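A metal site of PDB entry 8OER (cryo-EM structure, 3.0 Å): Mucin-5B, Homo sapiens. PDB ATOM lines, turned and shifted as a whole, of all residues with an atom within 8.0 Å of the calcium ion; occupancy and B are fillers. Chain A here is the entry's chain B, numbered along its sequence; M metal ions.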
ATOM      1  N   THR A  62      -4.436  10.162  12.321  1.00  0.00           N
ATOM      2  CA  THR A  62      -5.764   9.895  12.828  1.00  0.00           C
ATOM      3  C   THR A  62      -6.252  11.053  13.687  1.00  0.00           C
ATOM      4  O   THR A  62      -5.566  12.055  13.876  1.00  0.00           O
ATOM      5  CB  THR A  62      -5.790   8.600  13.629  1.00  0.00           C
ATOM      6  OG1 THR A  62      -5.568   8.892  15.019  1.00  0.00           O
ATOM      7  CG2 THR A  62      -4.719   7.655  13.145  1.00  0.00           C
ATOM      8  N   PHE A  63      -7.463  10.908  14.222  1.00  0.00           N
ATOM      9  CA  PHE A  63      -8.057  11.973  15.013  1.00  0.00           C
ATOM     10  C   PHE A  63      -7.241  12.258  16.260  1.00  0.00           C
ATOM     11  O   PHE A  63      -7.040  13.429  16.626  1.00  0.00           O
ATOM     12  CB  PHE A  63      -9.490  11.611  15.402  1.00  0.00           C
ATOM     13  CG  PHE A  63     -10.441  11.572  14.257  1.00  0.00           C
ATOM     14  CD1 PHE A  63     -10.428  12.561  13.306  1.00  0.00           C
ATOM     15  CD2 PHE A  63     -11.371  10.555  14.151  1.00  0.00           C
ATOM     16  CE1 PHE A  63     -11.307  12.540  12.266  1.00  0.00           C
ATOM     17  CE2 PHE A  63     -12.242  10.524  13.114  1.00  0.00           C
ATOM     18  CZ  PHE A  63     -12.218  11.522  12.165  1.00  0.00           C
ATOM     19  N   ASP A  64      -6.770  11.217  16.935  1.00  0.00           N
ATOM     20  CA  ASP A  64      -6.153  11.371  18.251  1.00  0.00           C
ATOM     21  C   ASP A  64      -4.639  11.517  18.177  1.00  0.00           C
ATOM     22  O   ASP A  64      -3.965  11.395  19.212  1.00  0.00           O
ATOM     23  CB  ASP A  64      -6.534  10.191  19.126  1.00  0.00           C
ATOM     24  CG  ASP A  64      -7.850   9.578  18.714  1.00  0.00           C
ATOM     25  OD1 ASP A  64      -8.769  10.349  18.359  1.00  0.00           O
ATOM     26  OD2 ASP A  64      -7.955   8.332  18.739  1.00  0.00           O
ATOM     27  N   ASP A  66      -2.277   9.840  16.158  1.00  0.00           N
ATOM     28  CA  ASP A  66      -1.431   8.792  15.633  1.00  0.00           C
ATOM     29  C   ASP A  66      -1.102   9.052  14.174  1.00  0.00           C
ATOM     30  O   ASP A  66      -1.936   9.499  13.384  1.00  0.00           O
ATOM     31  CB  ASP A  66      -2.108   7.430  15.752  1.00  0.00           C
ATOM     32  CG  ASP A  66      -2.408   7.066  17.182  1.00  0.00           C
ATOM     33  OD1 ASP A  66      -2.342   7.965  18.036  1.00  0.00           O
ATOM     34  OD2 ASP A  66      -2.712   5.887  17.449  1.00  0.00           O
ATOM     35  N   ASN A 176     -16.389   8.711  19.310  1.00  0.00           N
ATOM     36  CA  ASN A 176     -16.497   7.308  19.681  1.00  0.00           C
ATOM     37  C   ASN A 176     -17.438   6.514  18.783  1.00  0.00           C
ATOM     38  O   ASN A 176     -17.511   5.290  18.906  1.00  0.00           O
ATOM     39  CB  ASN A 176     -16.968   7.181  21.134  1.00  0.00           C
ATOM     40  CG  ASN A 176     -16.291   6.064  21.877  1.00  0.00           C
ATOM     41  OD1 ASN A 176     -15.506   5.301  21.313  1.00  0.00           O
ATOM     42  ND2 ASN A 176     -16.608   5.957  23.146  1.00  0.00           N
ATOM     43  N   CYS A 182      -9.054   7.047   9.993  1.00  0.00           N
ATOM     44  CA  CYS A 182      -8.972   8.235  10.835  1.00  0.00           C
ATOM     45  C   CYS A 182      -9.117   7.900  12.316  1.00  0.00           C
ATOM     46  O   CYS A 182      -8.954   8.800  13.150  1.00  0.00           O
ATOM     47  CB  CYS A 182     -10.047   9.249  10.435  1.00  0.00           C
ATOM     48  SG  CYS A 182      -9.761  10.030   8.837  1.00  0.00           S
ATOM     49  N   GLY A 183      -9.445   6.666  12.674  1.00  0.00           N
ATOM     50  CA  GLY A 183      -9.441   6.274  14.066  1.00  0.00           C
ATOM     51  C   GLY A 183     -10.797   6.317  14.725  1.00  0.00           C
ATOM     52  O   GLY A 183     -11.819   6.523  14.063  1.00  0.00           O
ATOM     53  N   ASP A 184     -10.833   6.137  16.046  1.00  0.00           N
ATOM     54  CA  ASP A 184     -12.093   6.013  16.774  1.00  0.00           C
ATOM     55  C   ASP A 184     -12.639   7.306  17.327  1.00  0.00           C
ATOM     56  O   ASP A 184     -13.789   7.313  17.775  1.00  0.00           O
ATOM     57  CB  ASP A 184     -11.955   5.018  17.930  1.00  0.00           C
ATOM     58  CG  ASP A 184     -10.749   5.315  18.787  1.00  0.00           C
ATOM     59  OD1 ASP A 184     -10.261   6.456  18.754  1.00  0.00           O
ATOM     60  OD2 ASP A 184     -10.288   4.407  19.514  1.00  0.00           O
ATOM     61  N   PHE A 185     -11.876   8.405  17.333  1.00  0.00           N
ATOM     62  CA  PHE A 185     -12.379   9.710  17.782  1.00  0.00           C
ATOM     63  C   PHE A 185     -12.871   9.665  19.227  1.00  0.00           C
ATOM     64  O   PHE A 185     -13.776  10.392  19.614  1.00  0.00           O
ATOM     65  CB  PHE A 185     -13.471  10.214  16.834  1.00  0.00           C
ATOM     66  CG  PHE A 185     -13.727  11.685  16.906  1.00  0.00           C
ATOM     67  CD1 PHE A 185     -12.902  12.513  17.634  1.00  0.00           C
ATOM     68  CD2 PHE A 185     -14.802  12.238  16.235  1.00  0.00           C
ATOM     69  CE1 PHE A 185     -13.167  13.865  17.700  1.00  0.00           C
ATOM     70  CE2 PHE A 185     -15.056  13.578  16.293  1.00  0.00           C
ATOM     71  CZ  PHE A 185     -14.232  14.396  17.022  1.00  0.00           C
ATOM     72  N   ASN A 186     -12.260   8.797  20.034  1.00  0.00           N
ATOM     73  CA  ASN A 186     -12.567   8.715  21.458  1.00  0.00           C
ATOM     74  C   ASN A 186     -11.613   9.536  22.306  1.00  0.00           C
ATOM     75  O   ASN A 186     -11.902   9.785  23.480  1.00  0.00           O
ATOM     76  CB  ASN A 186     -12.547   7.254  21.930  1.00  0.00           C
ATOM     77  CG  ASN A 186     -11.201   6.596  21.712  1.00  0.00           C
ATOM     78  OD1 ASN A 186     -10.238   7.228  21.273  1.00  0.00           O
ATOM     79  ND2 ASN A 186     -11.132   5.305  22.011  1.00  0.00           N
ATOM     80  N   GLY A 187     -10.479   9.949  21.750  1.00  0.00           N
ATOM     81  CA  GLY A 187      -9.532  10.795  22.442  1.00  0.00           C
ATOM     82  C   GLY A 187      -8.308  10.105  22.987  1.00  0.00           C
ATOM     83  O   GLY A 187      -7.384  10.793  23.437  1.00  0.00           O
ATOM     84  N   LEU A 188      -8.264   8.784  22.956  1.00  0.00           N
ATOM     85  CA  LEU A 188      -7.109   8.048  23.469  1.00  0.00           C
ATOM     86  C   LEU A 188      -6.301   7.513  22.305  1.00  0.00           C
ATOM     87  O   LEU A 188      -6.738   6.563  21.633  1.00  0.00           O
ATOM     88  CB  LEU A 188      -7.548   6.905  24.392  1.00  0.00           C
ATOM     89  CG  LEU A 188      -8.323   7.369  25.618  1.00  0.00           C
ATOM     90  CD1 LEU A 188      -8.904   6.171  26.361  1.00  0.00           C
ATOM     91  CD2 LEU A 188      -7.443   8.188  26.522  1.00  0.00           C
ATOM     92  N   PRO A 189      -5.133   8.074  22.035  1.00  0.00           N
ATOM     93  CA  PRO A 189      -4.400   7.724  20.805  1.00  0.00           C
ATOM     94  C   PRO A 189      -3.807   6.326  20.819  1.00  0.00           C
ATOM     95  O   PRO A 189      -3.953   5.571  19.859  1.00  0.00           O
ATOM     96  CB  PRO A 189      -3.288   8.769  20.742  1.00  0.00           C
ATOM     97  CG  PRO A 189      -3.237   9.415  22.057  1.00  0.00           C
ATOM     98  CD  PRO A 189      -4.505   9.171  22.780  1.00  0.00           C
ATOM     99  N   ALA A 190      -3.154   5.977  21.913  1.00  0.00           N
ATOM    100  CA  ALA A 190      -2.172   4.906  21.908  1.00  0.00           C
ATOM    101  C   ALA A 190      -2.706   3.564  22.372  1.00  0.00           C
ATOM    102  O   ALA A 190      -1.904   2.648  22.598  1.00  0.00           O
ATOM    103  CB  ALA A 190      -0.973   5.305  22.789  1.00  0.00           C
ATOM    104  N   PHE A 191      -4.016   3.394  22.541  1.00  0.00           N
ATOM    105  CA  PHE A 191      -4.458   2.171  23.201  1.00  0.00           C
ATOM    106  C   PHE A 191      -5.621   1.522  22.444  1.00  0.00           C
ATOM    107  O   PHE A 191      -5.770   0.301  22.490  1.00  0.00           O
ATOM    108  CB  PHE A 191      -4.804   2.526  24.685  1.00  0.00           C
ATOM    109  CG  PHE A 191      -5.846   1.647  25.356  1.00  0.00           C
ATOM    110  CD1 PHE A 191      -5.872   0.268  25.201  1.00  0.00           C
ATOM    111  CD2 PHE A 191      -6.827   2.224  26.145  1.00  0.00           C
ATOM    112  CE1 PHE A 191      -6.827  -0.519  25.834  1.00  0.00           C
ATOM    113  CE2 PHE A 191      -7.788   1.457  26.766  1.00  0.00           C
ATOM    114  CZ  PHE A 191      -7.784   0.085  26.616  1.00  0.00           C
ATOM    115  N   ASN A 192      -6.394   2.285  21.681  1.00  0.00           N
ATOM    116  CA  ASN A 192      -7.622   1.672  21.195  1.00  0.00           C
ATOM    117  C   ASN A 192      -7.705   1.494  19.674  1.00  0.00           C
ATOM    118  O   ASN A 192      -8.591   0.790  19.182  1.00  0.00           O
ATOM    119  CB  ASN A 192      -8.827   2.468  21.670  1.00  0.00           C
ATOM    120  CG  ASN A 192     -10.104   1.692  21.551  1.00  0.00           C
ATOM    121  OD1 ASN A 192     -10.105   0.469  21.627  1.00  0.00           O
ATOM    122  ND2 ASN A 192     -11.201   2.403  21.337  1.00  0.00           N
ATOM    123  N   GLU A 193      -6.772   2.088  18.924  1.00  0.00           N
ATOM    124  CA  GLU A 193      -6.831   1.990  17.465  1.00  0.00           C
ATOM    125  C   GLU A 193      -6.492   0.605  16.936  1.00  0.00           C
ATOM    126  O   GLU A 193      -7.229   0.077  16.097  1.00  0.00           O
ATOM    127  CB  GLU A 193      -5.877   2.988  16.821  1.00  0.00           C
ATOM    128  CG  GLU A 193      -6.092   4.446  17.178  1.00  0.00           C
ATOM    129  CD  GLU A 193      -7.516   4.886  17.003  1.00  0.00           C
ATOM    130  OE1 GLU A 193      -8.215   4.343  16.121  1.00  0.00           O
ATOM    131  OE2 GLU A 193      -7.938   5.794  17.746  1.00  0.00           O
ATOM    132  N   PHE A 194      -5.384   0.022  17.391  1.00  0.00           N
ATOM    133  CA  PHE A 194      -4.788  -1.138  16.748  1.00  0.00           C
ATOM    134  C   PHE A 194      -4.960  -2.409  17.569  1.00  0.00           C
ATOM    135  O   PHE A 194      -4.146  -3.328  17.491  1.00  0.00           O
ATOM    136  CB  PHE A 194      -3.306  -0.886  16.478  1.00  0.00           C
ATOM    137  CG  PHE A 194      -2.966   0.553  16.286  1.00  0.00           C
ATOM    138  CD1 PHE A 194      -3.369   1.220  15.144  1.00  0.00           C
ATOM    139  CD2 PHE A 194      -2.261   1.249  17.242  1.00  0.00           C
ATOM    140  CE1 PHE A 194      -3.061   2.543  14.962  1.00  0.00           C
ATOM    141  CE2 PHE A 194      -1.965   2.573  17.068  1.00  0.00           C
ATOM    142  CZ  PHE A 194      -2.360   3.219  15.929  1.00  0.00           C
HETATM  143 CA    CA M   1      -8.460   5.814  20.081  1.00  0.00          CA
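OD2 of Asp 184 sits close to ND2 of Asn 192 (2.9 Å). The backbone NH (N) of Asn 176 sits close to the backbone carbonyl oxygen (O) of Asp 184 (3.3 Å). ND2 of Asn 186 lies close to ND2 of Asn 192, 3.0 Å away. The backbone NH (N) of Asp 64 lies within hydrogen-bond range of the side-chain hydroxyl (OG1) of Thr 62, at 3.2 Å.
CB of Asn 192 touches the calcium ion, at 3.7 Å. Six residues have an atom within 4 Å of the calcium ion: Asp 64, Asp 184, Asn 186, Leu 188, Asn 192 and Glu 193.
OD1 of Asp 184 is bound to the calcium ion. The calcium ion is bound by OD2 of Asp 184, 2.4 Å away. OE2 of Glu 193 is bound to the calcium ion, 2.4 Å away. O of Leu 188 is bound to the calcium ion, at 2.4 Å. OD1 of Asn 186 is bound to the calcium ion (2.6 Å). The calcium ion is bound by OD2 of Asp 64.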
